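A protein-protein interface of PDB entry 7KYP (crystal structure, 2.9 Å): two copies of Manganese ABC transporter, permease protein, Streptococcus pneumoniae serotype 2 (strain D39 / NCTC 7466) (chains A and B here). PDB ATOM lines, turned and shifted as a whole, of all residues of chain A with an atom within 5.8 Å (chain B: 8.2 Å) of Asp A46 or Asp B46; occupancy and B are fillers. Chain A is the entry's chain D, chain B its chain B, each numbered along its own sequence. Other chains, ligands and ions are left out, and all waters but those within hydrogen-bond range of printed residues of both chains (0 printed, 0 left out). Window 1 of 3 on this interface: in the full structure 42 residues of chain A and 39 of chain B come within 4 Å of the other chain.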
ATOM      1  N   MET A  41     -30.808 -10.189 -22.942  1.00  0.00           N
ATOM      2  CA  MET A  41     -29.445 -10.629 -23.238  1.00  0.00           C
ATOM      3  C   MET A  41     -28.860 -11.490 -22.114  1.00  0.00           C
ATOM      4  O   MET A  41     -27.650 -11.714 -22.067  1.00  0.00           O
ATOM      5  CB  MET A  41     -28.544  -9.412 -23.474  1.00  0.00           C
ATOM      6  CG  MET A  41     -28.939  -8.557 -24.668  1.00  0.00           C
ATOM      7  SD  MET A  41     -28.069  -6.977 -24.706  1.00  0.00           S
ATOM      8  CE  MET A  41     -26.362  -7.514 -24.795  1.00  0.00           C
ATOM      9  N   SER A  42     -29.720 -11.976 -21.218  1.00  0.00           N
ATOM     10  CA  SER A  42     -29.288 -12.798 -20.085  1.00  0.00           C
ATOM     11  C   SER A  42     -28.503 -14.027 -20.533  1.00  0.00           C
ATOM     12  O   SER A  42     -27.499 -14.388 -19.918  1.00  0.00           O
ATOM     13  CB  SER A  42     -30.498 -13.238 -19.256  1.00  0.00           C
ATOM     14  OG  SER A  42     -31.248 -12.119 -18.818  1.00  0.00           O
ATOM     15  N   LEU A  43     -28.972 -14.667 -21.603  1.00  0.00           N
ATOM     16  CA  LEU A  43     -28.283 -15.813 -22.199  1.00  0.00           C
ATOM     17  C   LEU A  43     -26.917 -15.413 -22.751  1.00  0.00           C
ATOM     18  O   LEU A  43     -25.922 -16.097 -22.520  1.00  0.00           O
ATOM     19  CB  LEU A  43     -29.137 -16.416 -23.321  1.00  0.00           C
ATOM     20  CG  LEU A  43     -28.535 -17.559 -24.145  1.00  0.00           C
ATOM     21  CD1 LEU A  43     -28.127 -18.721 -23.251  1.00  0.00           C
ATOM     22  CD2 LEU A  43     -29.526 -18.014 -25.206  1.00  0.00           C
ATOM     23  N   MET A  44     -26.883 -14.299 -23.480  1.00  0.00           N
ATOM     24  CA  MET A  44     -25.648 -13.803 -24.086  1.00  0.00           C
ATOM     25  C   MET A  44     -24.665 -13.305 -23.023  1.00  0.00           C
ATOM     26  O   MET A  44     -23.452 -13.361 -23.222  1.00  0.00           O
ATOM     27  CB  MET A  44     -25.958 -12.678 -25.079  1.00  0.00           C
ATOM     28  CG  MET A  44     -24.878 -12.447 -26.123  1.00  0.00           C
ATOM     29  SD  MET A  44     -24.839 -13.747 -27.375  1.00  0.00           S
ATOM     30  CE  MET A  44     -23.572 -13.114 -28.472  1.00  0.00           C
ATOM     31  N   GLY A  45     -25.193 -12.817 -21.903  1.00  0.00           N
ATOM     32  CA  GLY A  45     -24.367 -12.393 -20.775  1.00  0.00           C
ATOM     33  C   GLY A  45     -23.533 -13.525 -20.201  1.00  0.00           C
ATOM     34  O   GLY A  45     -22.358 -13.340 -19.881  1.00  0.00           O
ATOM     35  N   ASP A  46     -24.147 -14.699 -20.081  1.00  0.00           N
ATOM     36  CA  ASP A  46     -23.469 -15.884 -19.557  1.00  0.00           C
ATOM     37  C   ASP A  46     -22.366 -16.363 -20.504  1.00  0.00           C
ATOM     38  O   ASP A  46     -21.297 -16.775 -20.057  1.00  0.00           O
ATOM     39  CB  ASP A  46     -24.485 -17.009 -19.315  1.00  0.00           C
ATOM     40  CG  ASP A  46     -23.939 -18.118 -18.430  1.00  0.00           C
ATOM     41  OD1 ASP A  46     -23.305 -17.810 -17.399  1.00  0.00           O
ATOM     42  OD2 ASP A  46     -24.162 -19.304 -18.759  1.00  0.00           O
ATOM     43  N   ALA A  47     -22.633 -16.296 -21.808  1.00  0.00           N
ATOM     44  CA  ALA A  47     -21.689 -16.759 -22.830  1.00  0.00           C
ATOM     45  C   ALA A  47     -20.453 -15.871 -22.938  1.00  0.00           C
ATOM     46  O   ALA A  47     -19.336 -16.373 -23.072  1.00  0.00           O
ATOM     47  CB  ALA A  47     -22.385 -16.849 -24.179  1.00  0.00           C
ATOM     48  N   ILE A  48     -20.661 -14.557 -22.890  1.00  0.00           N
ATOM     49  CA  ILE A  48     -19.566 -13.585 -22.962  1.00  0.00           C
ATOM     50  C   ILE A  48     -18.606 -13.749 -21.780  1.00  0.00           C
ATOM     51  O   ILE A  48     -17.392 -13.637 -21.945  1.00  0.00           O
ATOM     52  CB  ILE A  48     -20.103 -12.132 -23.014  1.00  0.00           C
ATOM     53  CG1 ILE A  48     -20.814 -11.864 -24.349  1.00  0.00           C
ATOM     54  CG2 ILE A  48     -18.986 -11.112 -22.803  1.00  0.00           C
ATOM     55  CD1 ILE A  48     -19.890 -11.682 -25.537  1.00  0.00           C
ATOM     56  N   SER A  49     -19.156 -14.017 -20.599  1.00  0.00           N
ATOM     57  CA  SER A  49     -18.351 -14.271 -19.404  1.00  0.00           C
ATOM     58  C   SER A  49     -17.428 -15.475 -19.585  1.00  0.00           C
ATOM     59  O   SER A  49     -16.268 -15.439 -19.180  1.00  0.00           O
ATOM     60  CB  SER A  49     -19.262 -14.501 -18.199  1.00  0.00           C
ATOM     61  OG  SER A  49     -20.086 -13.372 -17.968  1.00  0.00           O
ATOM     62  N   HIS A  50     -17.953 -16.534 -20.196  1.00  0.00           N
ATOM     63  CA  HIS A  50     -17.170 -17.737 -20.491  1.00  0.00           C
ATOM     64  C   HIS A  50     -16.134 -17.468 -21.585  1.00  0.00           C
ATOM     65  O   HIS A  50     -15.021 -17.991 -21.535  1.00  0.00           O
ATOM     66  CB  HIS A  50     -18.092 -18.883 -20.920  1.00  0.00           C
ATOM     67  CG  HIS A  50     -18.956 -19.412 -19.816  1.00  0.00           C
ATOM     68  ND1 HIS A  50     -19.379 -20.723 -19.770  1.00  0.00           N
ATOM     69  CD2 HIS A  50     -19.465 -18.814 -18.713  1.00  0.00           C
ATOM     70  CE1 HIS A  50     -20.120 -20.906 -18.692  1.00  0.00           C
ATOM     71  NE2 HIS A  50     -20.187 -19.764 -18.034  1.00  0.00           N
ATOM     72  N   ALA A  51     -16.512 -16.648 -22.566  1.00  0.00           N
ATOM     73  CA  ALA A  51     -15.621 -16.279 -23.670  1.00  0.00           C
ATOM     74  C   ALA A  51     -14.461 -15.378 -23.235  1.00  0.00           C
ATOM     75  O   ALA A  51     -13.453 -15.286 -23.935  1.00  0.00           O
ATOM     76  CB  ALA A  51     -16.415 -15.606 -24.780  1.00  0.00           C
ATOM     77  N   SER A 100     -19.597 -20.909 -26.068  1.00  0.00           N
ATOM     78  CA  SER A 100     -19.252 -20.562 -24.687  1.00  0.00           C
ATOM     79  C   SER A 100     -18.567 -21.725 -23.972  1.00  0.00           C
ATOM     80  O   SER A 100     -17.586 -21.521 -23.254  1.00  0.00           O
ATOM     81  CB  SER A 100     -20.493 -20.112 -23.908  1.00  0.00           C
ATOM     82  OG  SER A 100     -21.485 -21.122 -23.887  1.00  0.00           O
ATOM     83  N   THR A 198     -15.756 -15.919 -12.687  1.00  0.00           N
ATOM     84  CA  THR A 198     -16.247 -15.987 -14.068  1.00  0.00           C
ATOM     85  C   THR A 198     -17.593 -16.708 -14.215  1.00  0.00           C
ATOM     86  O   THR A 198     -18.423 -16.314 -15.036  1.00  0.00           O
ATOM     87  CB  THR A 198     -15.214 -16.686 -14.981  1.00  0.00           C
ATOM     88  OG1 THR A 198     -13.975 -15.966 -14.943  1.00  0.00           O
ATOM     89  CG2 THR A 198     -15.701 -16.763 -16.422  1.00  0.00           C
ATOM     90  N   ILE A 199     -17.805 -17.754 -13.422  1.00  0.00           N
ATOM     91  CA  ILE A 199     -18.995 -18.598 -13.562  1.00  0.00           C
ATOM     92  C   ILE A 199     -20.255 -17.945 -12.980  1.00  0.00           C
ATOM     93  O   ILE A 199     -21.353 -18.151 -13.502  1.00  0.00           O
ATOM     94  CB  ILE A 199     -18.782 -19.991 -12.916  1.00  0.00           C
ATOM     95  CG1 ILE A 199     -17.549 -20.691 -13.508  1.00  0.00           C
ATOM     96  CG2 ILE A 199     -20.016 -20.866 -13.090  1.00  0.00           C
ATOM     97  CD1 ILE A 199     -17.585 -20.881 -15.011  1.00  0.00           C
ATOM     98  N   VAL A 202     -23.015 -13.669 -14.145  1.00  0.00           N
ATOM     99  CA  VAL A 202     -24.404 -13.598 -14.604  1.00  0.00           C
ATOM    100  C   VAL A 202     -25.403 -13.415 -13.457  1.00  0.00           C
ATOM    101  O   VAL A 202     -26.367 -12.665 -13.592  1.00  0.00           O
ATOM    102  CB  VAL A 202     -24.783 -14.844 -15.448  1.00  0.00           C
ATOM    103  CG1 VAL A 202     -24.684 -16.128 -14.625  1.00  0.00           C
ATOM    104  CG2 VAL A 202     -26.173 -14.691 -16.053  1.00  0.00           C
ATOM    105  N   ILE B  36     -32.382 -32.688 -27.357  1.00  0.00           N
ATOM    106  CA  ILE B  36     -32.221 -31.396 -26.688  1.00  0.00           C
ATOM    107  C   ILE B  36     -32.162 -30.250 -27.700  1.00  0.00           C
ATOM    108  O   ILE B  36     -32.904 -29.275 -27.574  1.00  0.00           O
ATOM    109  CB  ILE B  36     -30.958 -31.370 -25.789  1.00  0.00           C
ATOM    110  CG1 ILE B  36     -31.051 -32.427 -24.676  1.00  0.00           C
ATOM    111  CG2 ILE B  36     -30.745 -29.990 -25.180  1.00  0.00           C
ATOM    112  CD1 ILE B  36     -32.292 -32.335 -23.810  1.00  0.00           C
ATOM    113  N   MET B  41     -33.883 -26.931 -26.579  1.00  0.00           N
ATOM    114  CA  MET B  41     -33.704 -26.997 -25.127  1.00  0.00           C
ATOM    115  C   MET B  41     -32.232 -26.881 -24.718  1.00  0.00           C
ATOM    116  O   MET B  41     -31.854 -27.310 -23.626  1.00  0.00           O
ATOM    117  CB  MET B  41     -34.286 -28.310 -24.594  1.00  0.00           C
ATOM    118  CG  MET B  41     -35.791 -28.448 -24.765  1.00  0.00           C
ATOM    119  SD  MET B  41     -36.372 -30.122 -24.427  1.00  0.00           S
ATOM    120  CE  MET B  41     -35.779 -30.368 -22.753  1.00  0.00           C
ATOM    121  N   SER B  42     -31.410 -26.292 -25.584  1.00  0.00           N
ATOM    122  CA  SER B  42     -29.972 -26.160 -25.328  1.00  0.00           C
ATOM    123  C   SER B  42     -29.687 -25.382 -24.043  1.00  0.00           C
ATOM    124  O   SER B  42     -28.774 -25.727 -23.290  1.00  0.00           O
ATOM    125  CB  SER B  42     -29.284 -25.477 -26.510  1.00  0.00           C
ATOM    126  OG  SER B  42     -29.552 -26.167 -27.720  1.00  0.00           O
ATOM    127  N   LEU B  43     -30.471 -24.332 -23.806  1.00  0.00           N
ATOM    128  CA  LEU B  43     -30.394 -23.557 -22.567  1.00  0.00           C
ATOM    129  C   LEU B  43     -30.775 -24.406 -21.355  1.00  0.00           C
ATOM    130  O   LEU B  43     -30.094 -24.377 -20.329  1.00  0.00           O
ATOM    131  CB  LEU B  43     -31.313 -22.333 -22.651  1.00  0.00           C
ATOM    132  CG  LEU B  43     -31.511 -21.499 -21.381  1.00  0.00           C
ATOM    133  CD1 LEU B  43     -30.177 -21.039 -20.808  1.00  0.00           C
ATOM    134  CD2 LEU B  43     -32.419 -20.313 -21.674  1.00  0.00           C
ATOM    135  N   MET B  44     -31.864 -25.159 -21.486  1.00  0.00           N
ATOM    136  CA  MET B  44     -32.375 -25.990 -20.392  1.00  0.00           C
ATOM    137  C   MET B  44     -31.397 -27.108 -20.027  1.00  0.00           C
ATOM    138  O   MET B  44     -31.336 -27.530 -18.871  1.00  0.00           O
ATOM    139  CB  MET B  44     -33.739 -26.588 -20.761  1.00  0.00           C
ATOM    140  CG  MET B  44     -34.693 -26.723 -19.586  1.00  0.00           C
ATOM    141  SD  MET B  44     -35.414 -25.137 -19.116  1.00  0.00           S
ATOM    142  CE  MET B  44     -36.487 -25.637 -17.772  1.00  0.00           C
ATOM    143  N   GLY B  45     -30.639 -27.587 -21.014  1.00  0.00           N
ATOM    144  CA  GLY B  45     -29.590 -28.576 -20.778  1.00  0.00           C
ATOM    145  C   GLY B  45     -28.512 -28.062 -19.843  1.00  0.00           C
ATOM    146  O   GLY B  45     -28.036 -28.792 -18.972  1.00  0.00           O
ATOM    147  N   ASP B  46     -28.129 -26.799 -20.025  1.00  0.00           N
ATOM    148  CA  ASP B  46     -27.142 -26.148 -19.165  1.00  0.00           C
ATOM    149  C   ASP B  46     -27.720 -25.844 -17.783  1.00  0.00           C
ATOM    150  O   ASP B  46     -27.020 -25.958 -16.778  1.00  0.00           O
ATOM    151  CB  ASP B  46     -26.650 -24.848 -19.814  1.00  0.00           C
ATOM    152  CG  ASP B  46     -25.436 -24.258 -19.110  1.00  0.00           C
ATOM    153  OD1 ASP B  46     -24.494 -25.015 -18.790  1.00  0.00           O
ATOM    154  OD2 ASP B  46     -25.418 -23.030 -18.887  1.00  0.00           O
ATOM    155  N   ALA B  47     -28.993 -25.455 -17.741  1.00  0.00           N
ATOM    156  CA  ALA B  47     -29.655 -25.085 -16.488  1.00  0.00           C
ATOM    157  C   ALA B  47     -29.839 -26.277 -15.551  1.00  0.00           C
ATOM    158  O   ALA B  47     -29.570 -26.176 -14.354  1.00  0.00           O
ATOM    159  CB  ALA B  47     -30.999 -24.432 -16.776  1.00  0.00           C
ATOM    160  N   ILE B  48     -30.300 -27.398 -16.101  1.00  0.00           N
ATOM    161  CA  ILE B  48     -30.517 -28.619 -15.316  1.00  0.00           C
ATOM    162  C   ILE B  48     -29.192 -29.208 -14.817  1.00  0.00           C
ATOM    163  O   ILE B  48     -29.131 -29.742 -13.710  1.00  0.00           O
ATOM    164  CB  ILE B  48     -31.318 -29.674 -16.121  1.00  0.00           C
ATOM    165  CG1 ILE B  48     -32.747 -29.173 -16.391  1.00  0.00           C
ATOM    166  CG2 ILE B  48     -31.359 -31.017 -15.399  1.00  0.00           C
ATOM    167  CD1 ILE B  48     -33.588 -28.934 -15.151  1.00  0.00           C
ATOM    168  N   SER B  49     -28.137 -29.097 -15.623  1.00  0.00           N
ATOM    169  CA  SER B  49     -26.795 -29.514 -15.207  1.00  0.00           C
ATOM    170  C   SER B  49     -26.352 -28.806 -13.924  1.00  0.00           C
ATOM    171  O   SER B  49     -25.743 -29.420 -13.046  1.00  0.00           O
ATOM    172  CB  SER B  49     -25.783 -29.238 -16.321  1.00  0.00           C
ATOM    173  OG  SER B  49     -26.108 -29.963 -17.494  1.00  0.00           O
ATOM    174  N   HIS B  50     -26.667 -27.517 -13.830  1.00  0.00           N
ATOM    175  CA  HIS B  50     -26.365 -26.719 -12.641  1.00  0.00           C
ATOM    176  C   HIS B  50     -27.341 -27.023 -11.504  1.00  0.00           C
ATOM    177  O   HIS B  50     -26.945 -27.082 -10.340  1.00  0.00           O
ATOM    178  CB  HIS B  50     -26.416 -25.227 -12.980  1.00  0.00           C
ATOM    179  CG  HIS B  50     -25.307 -24.772 -13.879  1.00  0.00           C
ATOM    180  ND1 HIS B  50     -24.746 -23.516 -13.786  1.00  0.00           N
ATOM    181  CD2 HIS B  50     -24.646 -25.406 -14.876  1.00  0.00           C
ATOM    182  CE1 HIS B  50     -23.794 -23.394 -14.694  1.00  0.00           C
ATOM    183  NE2 HIS B  50     -23.713 -24.527 -15.369  1.00  0.00           N
ATOM    184  N   ALA B  51     -28.613 -27.210 -11.850  1.00  0.00           N
ATOM    185  CA  ALA B  51     -29.663 -27.507 -10.867  1.00  0.00           C
ATOM    186  C   ALA B  51     -29.486 -28.864 -10.185  1.00  0.00           C
ATOM    187  O   ALA B  51     -29.969 -29.066  -9.071  1.00  0.00           O
ATOM    188  CB  ALA B  51     -31.033 -27.431 -11.525  1.00  0.00           C
ATOM    189  N   VAL B  52     -28.807 -29.789 -10.858  1.00  0.00           N
ATOM    190  CA  VAL B  52     -28.549 -31.126 -10.316  1.00  0.00           C
ATOM    191  C   VAL B  52     -27.528 -31.104  -9.170  1.00  0.00           C
ATOM    192  O   VAL B  52     -27.660 -31.865  -8.212  1.00  0.00           O
ATOM    193  CB  VAL B  52     -28.089 -32.091 -11.438  1.00  0.00           C
ATOM    194  CG1 VAL B  52     -27.432 -33.343 -10.876  1.00  0.00           C
ATOM    195  CG2 VAL B  52     -29.268 -32.472 -12.326  1.00  0.00           C
ATOM    196  N   ILE B  96     -34.421 -18.608 -15.976  1.00  0.00           N
ATOM    197  CA  ILE B  96     -33.515 -19.750 -16.114  1.00  0.00           C
ATOM    198  C   ILE B  96     -32.103 -19.393 -15.632  1.00  0.00           C
ATOM    199  O   ILE B  96     -31.415 -20.230 -15.047  1.00  0.00           O
ATOM    200  CB  ILE B  96     -33.464 -20.258 -17.574  1.00  0.00           C
ATOM    201  CG1 ILE B  96     -34.841 -20.779 -18.006  1.00  0.00           C
ATOM    202  CG2 ILE B  96     -32.424 -21.365 -17.731  1.00  0.00           C
ATOM    203  CD1 ILE B  96     -35.040 -20.818 -19.506  1.00  0.00           C
ATOM    204  N   GLY B  97     -31.678 -18.156 -15.882  1.00  0.00           N
ATOM    205  CA  GLY B  97     -30.370 -17.682 -15.435  1.00  0.00           C
ATOM    206  C   GLY B  97     -30.263 -17.540 -13.926  1.00  0.00           C
ATOM    207  O   GLY B  97     -29.249 -17.911 -13.332  1.00  0.00           O
ATOM    208  N   SER B 100     -30.614 -21.156 -12.124  1.00  0.00           N
ATOM    209  CA  SER B 100     -29.481 -22.040 -12.407  1.00  0.00           C
ATOM    210  C   SER B 100     -28.247 -21.645 -11.596  1.00  0.00           C
ATOM    211  O   SER B 100     -27.588 -22.502 -11.007  1.00  0.00           O
ATOM    212  CB  SER B 100     -29.149 -22.035 -13.901  1.00  0.00           C
ATOM    213  OG  SER B 100     -28.868 -20.724 -14.360  1.00  0.00           O
ATOM    214  N   SER B 101     -27.944 -20.348 -11.569  1.00  0.00           N
ATOM    215  CA  SER B 101     -26.794 -19.834 -10.820  1.00  0.00           C
ATOM    216  C   SER B 101     -27.004 -19.912  -9.306  1.00  0.00           C
ATOM    217  O   SER B 101     -26.051 -20.128  -8.557  1.00  0.00           O
ATOM    218  CB  SER B 101     -26.488 -18.390 -11.228  1.00  0.00           C
ATOM    219  OG  SER B 101     -27.549 -17.520 -10.874  1.00  0.00           O
ATOM    220  N   LEU B 104     -26.534 -23.551  -8.470  1.00  0.00           N
ATOM    221  CA  LEU B 104     -25.092 -23.792  -8.577  1.00  0.00           C
ATOM    222  C   LEU B 104     -24.356 -23.305  -7.330  1.00  0.00           C
ATOM    223  O   LEU B 104     -23.513 -24.019  -6.783  1.00  0.00           O
ATOM    224  CB  LEU B 104     -24.522 -23.099  -9.819  1.00  0.00           C
ATOM    225  CG  LEU B 104     -23.000 -23.152 -10.004  1.00  0.00           C
ATOM    226  CD1 LEU B 104     -22.514 -24.587 -10.128  1.00  0.00           C
ATOM    227  CD2 LEU B 104     -22.578 -22.339 -11.215  1.00  0.00           C
ATOM    228  N   LEU B 185     -32.380 -36.440 -18.897  1.00  0.00           N
ATOM    229  CA  LEU B 185     -31.337 -35.409 -18.851  1.00  0.00           C
ATOM    230  C   LEU B 185     -30.604 -35.361 -17.508  1.00  0.00           C
ATOM    231  O   LEU B 185     -29.386 -35.171 -17.473  1.00  0.00           O
ATOM    232  CB  LEU B 185     -31.944 -34.034 -19.158  1.00  0.00           C
ATOM    233  CG  LEU B 185     -31.033 -32.801 -19.096  1.00  0.00           C
ATOM    234  CD1 LEU B 185     -29.835 -32.949 -20.022  1.00  0.00           C
ATOM    235  CD2 LEU B 185     -31.822 -31.546 -19.439  1.00  0.00           C
ATOM    236  N   SER B 189     -26.701 -36.025 -16.689  1.00  0.00           N
ATOM    237  CA  SER B 189     -25.920 -34.986 -16.018  1.00  0.00           C
ATOM    238  C   SER B 189     -25.034 -35.545 -14.905  1.00  0.00           C
ATOM    239  O   SER B 189     -23.830 -35.287 -14.883  1.00  0.00           O
ATOM    240  CB  SER B 189     -26.845 -33.905 -15.455  1.00  0.00           C
ATOM    241  OG  SER B 189     -27.595 -33.292 -16.489  1.00  0.00           O
ATOM    242  N   THR B 198     -19.632 -30.956 -13.795  1.00  0.00           N
ATOM    243  CA  THR B 198     -20.844 -30.123 -13.795  1.00  0.00           C
ATOM    244  C   THR B 198     -20.793 -28.933 -14.755  1.00  0.00           C
ATOM    245  O   THR B 198     -21.790 -28.614 -15.406  1.00  0.00           O
ATOM    246  CB  THR B 198     -21.139 -29.581 -12.377  1.00  0.00           C
ATOM    247  OG1 THR B 198     -21.217 -30.672 -11.450  1.00  0.00           O
ATOM    248  CG2 THR B 198     -22.450 -28.799 -12.344  1.00  0.00           C
ATOM    249  N   ILE B 199     -19.633 -28.286 -14.843  1.00  0.00           N
ATOM    250  CA  ILE B 199     -19.489 -27.048 -15.612  1.00  0.00           C
ATOM    251  C   ILE B 199     -19.538 -27.282 -17.130  1.00  0.00           C
ATOM    252  O   ILE B 199     -19.986 -26.407 -17.872  1.00  0.00           O
ATOM    253  CB  ILE B 199     -18.184 -26.301 -15.235  1.00  0.00           C
ATOM    254  CG1 ILE B 199     -18.145 -25.977 -13.732  1.00  0.00           C
ATOM    255  CG2 ILE B 199     -18.029 -25.020 -16.047  1.00  0.00           C
ATOM    256  CD1 ILE B 199     -19.257 -25.068 -13.246  1.00  0.00           C
ATOM    257  N   LEU B 200     -19.092 -28.454 -17.582  1.00  0.00           N
ATOM    258  CA  LEU B 200     -19.004 -28.751 -19.019  1.00  0.00           C
ATOM    259  C   LEU B 200     -19.947 -29.871 -19.497  1.00  0.00           C
ATOM    260  O   LEU B 200     -19.713 -30.465 -20.551  1.00  0.00           O
ATOM    261  CB  LEU B 200     -17.552 -29.093 -19.385  1.00  0.00           C
ATOM    262  CG  LEU B 200     -16.538 -27.950 -19.276  1.00  0.00           C
ATOM    263  CD1 LEU B 200     -15.115 -28.487 -19.325  1.00  0.00           C
ATOM    264  CD2 LEU B 200     -16.755 -26.916 -20.372  1.00  0.00           C
ATOM    265  N   ILE B 201     -21.015 -30.143 -18.747  1.00  0.00           N
ATOM    266  CA  ILE B 201     -21.997 -31.160 -19.148  1.00  0.00           C
ATOM    267  C   ILE B 201     -22.693 -30.759 -20.448  1.00  0.00           C
ATOM    268  O   ILE B 201     -22.823 -31.571 -21.364  1.00  0.00           O
ATOM    269  CB  ILE B 201     -23.060 -31.410 -18.050  1.00  0.00           C
ATOM    270  CG1 ILE B 201     -22.421 -32.129 -16.858  1.00  0.00           C
ATOM    271  CG2 ILE B 201     -24.218 -32.241 -18.594  1.00  0.00           C
ATOM    272  CD1 ILE B 201     -23.296 -32.208 -15.624  1.00  0.00           C
ATOM    273  N   VAL B 202     -23.133 -29.504 -20.514  1.00  0.00           N
ATOM    274  CA  VAL B 202     -23.830 -28.968 -21.689  1.00  0.00           C
ATOM    275  C   VAL B 202     -23.100 -29.262 -23.006  1.00  0.00           C
ATOM    276  O   VAL B 202     -23.741 -29.514 -24.025  1.00  0.00           O
ATOM    277  CB  VAL B 202     -24.077 -27.443 -21.552  1.00  0.00           C
ATOM    278  CG1 VAL B 202     -22.764 -26.664 -21.566  1.00  0.00           C
ATOM    279  CG2 VAL B 202     -25.012 -26.943 -22.645  1.00  0.00           C
ATOM    280  N   ALA B 203     -21.768 -29.233 -22.976  1.00  0.00           N
ATOM    281  CA  ALA B 203     -20.947 -29.479 -24.163  1.00  0.00           C
ATOM    282  C   ALA B 203     -21.149 -30.884 -24.726  1.00  0.00           C
ATOM    283  O   ALA B 203     -21.247 -31.058 -25.938  1.00  0.00           O
ATOM    284  CB  ALA B 203     -19.477 -29.256 -23.842  1.00  0.00           C
ATOM    285  N   LEU B 205     -23.755 -32.741 -24.482  1.00  0.00           N
ATOM    286  CA  LEU B 205     -25.097 -32.876 -25.038  1.00  0.00           C
ATOM    287  C   LEU B 205     -25.180 -32.263 -26.433  1.00  0.00           C
ATOM    288  O   LEU B 205     -25.514 -32.949 -27.400  1.00  0.00           O
ATOM    289  CB  LEU B 205     -26.129 -32.210 -24.122  1.00  0.00           C
ATOM    290  CG  LEU B 205     -26.230 -32.756 -22.695  1.00  0.00           C
ATOM    291  CD1 LEU B 205     -27.192 -31.911 -21.875  1.00  0.00           C
ATOM    292  CD2 LEU B 205     -26.663 -34.214 -22.697  1.00  0.00           C
ATOM    293  N   ILE B 206     -24.855 -30.977 -26.536  1.00  0.00           N
ATOM    294  CA  ILE B 206     -25.144 -30.204 -27.748  1.00  0.00           C
ATOM    295  C   ILE B 206     -24.073 -30.287 -28.842  1.00  0.00           C
ATOM    296  O   ILE B 206     -24.409 -30.264 -30.026  1.00  0.00           O
ATOM    297  CB  ILE B 206     -25.449 -28.719 -27.422  1.00  0.00           C
ATOM    298  CG1 ILE B 206     -24.177 -27.949 -27.038  1.00  0.00           C
ATOM    299  CG2 ILE B 206     -26.502 -28.625 -26.324  1.00  0.00           C
ATOM    300  CD1 ILE B 206     -24.427 -26.511 -26.640  1.00  0.00           C
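Of the printed residues of chain B, Leu A43 touches Leu B43. No residue of chain B comes within 4 Å of Gly A45. Asp A46 touches one residue of chain B. No residue of chain B comes within 4 Å of Ala A47. Of the printed residues of chain B, Ile A199 touches Leu B104 (3.5 Å). Ile B36 touches none of the printed residues of chain A. Printed residues of chain A within 4 Å of Leu B43: Leu A43 (3.9 Å). Asp B46 touches just one residue of chain A: Asp A46. Of the printed residues of chain A, Leu B104 touches Ile A199. The nearest residue of chain B that does not touch Asp A46 is His B50 (5.8 Å). The nearest printed residue of chain A that does not touch Leu B104 is Val A202 (7.4 Å).
Among the printed residues, merely in contact across the chains: Ile A199 with Leu B104, Asp A46 with Asp B46 and Leu A43 with Leu B43.
Printed residues of chain A that touch a printed residue of chain B: Leu A43, Asp A46 and Ile A199. Hydrophobic or aromatic side chains of chain A within 4 Å of the printed part of chain B: Leu A43 and Ile A199. Among the printed residues, 3 pairs touch across the chains. Among the printed residues, no Asp or Glu carboxylate lies within 4 Å of a Lys or Arg side-chain nitrogen of the other chain.
Leu A43 touches its own counterpart, Leu B43. Asp A46 touches its own counterpart, Asp B46.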
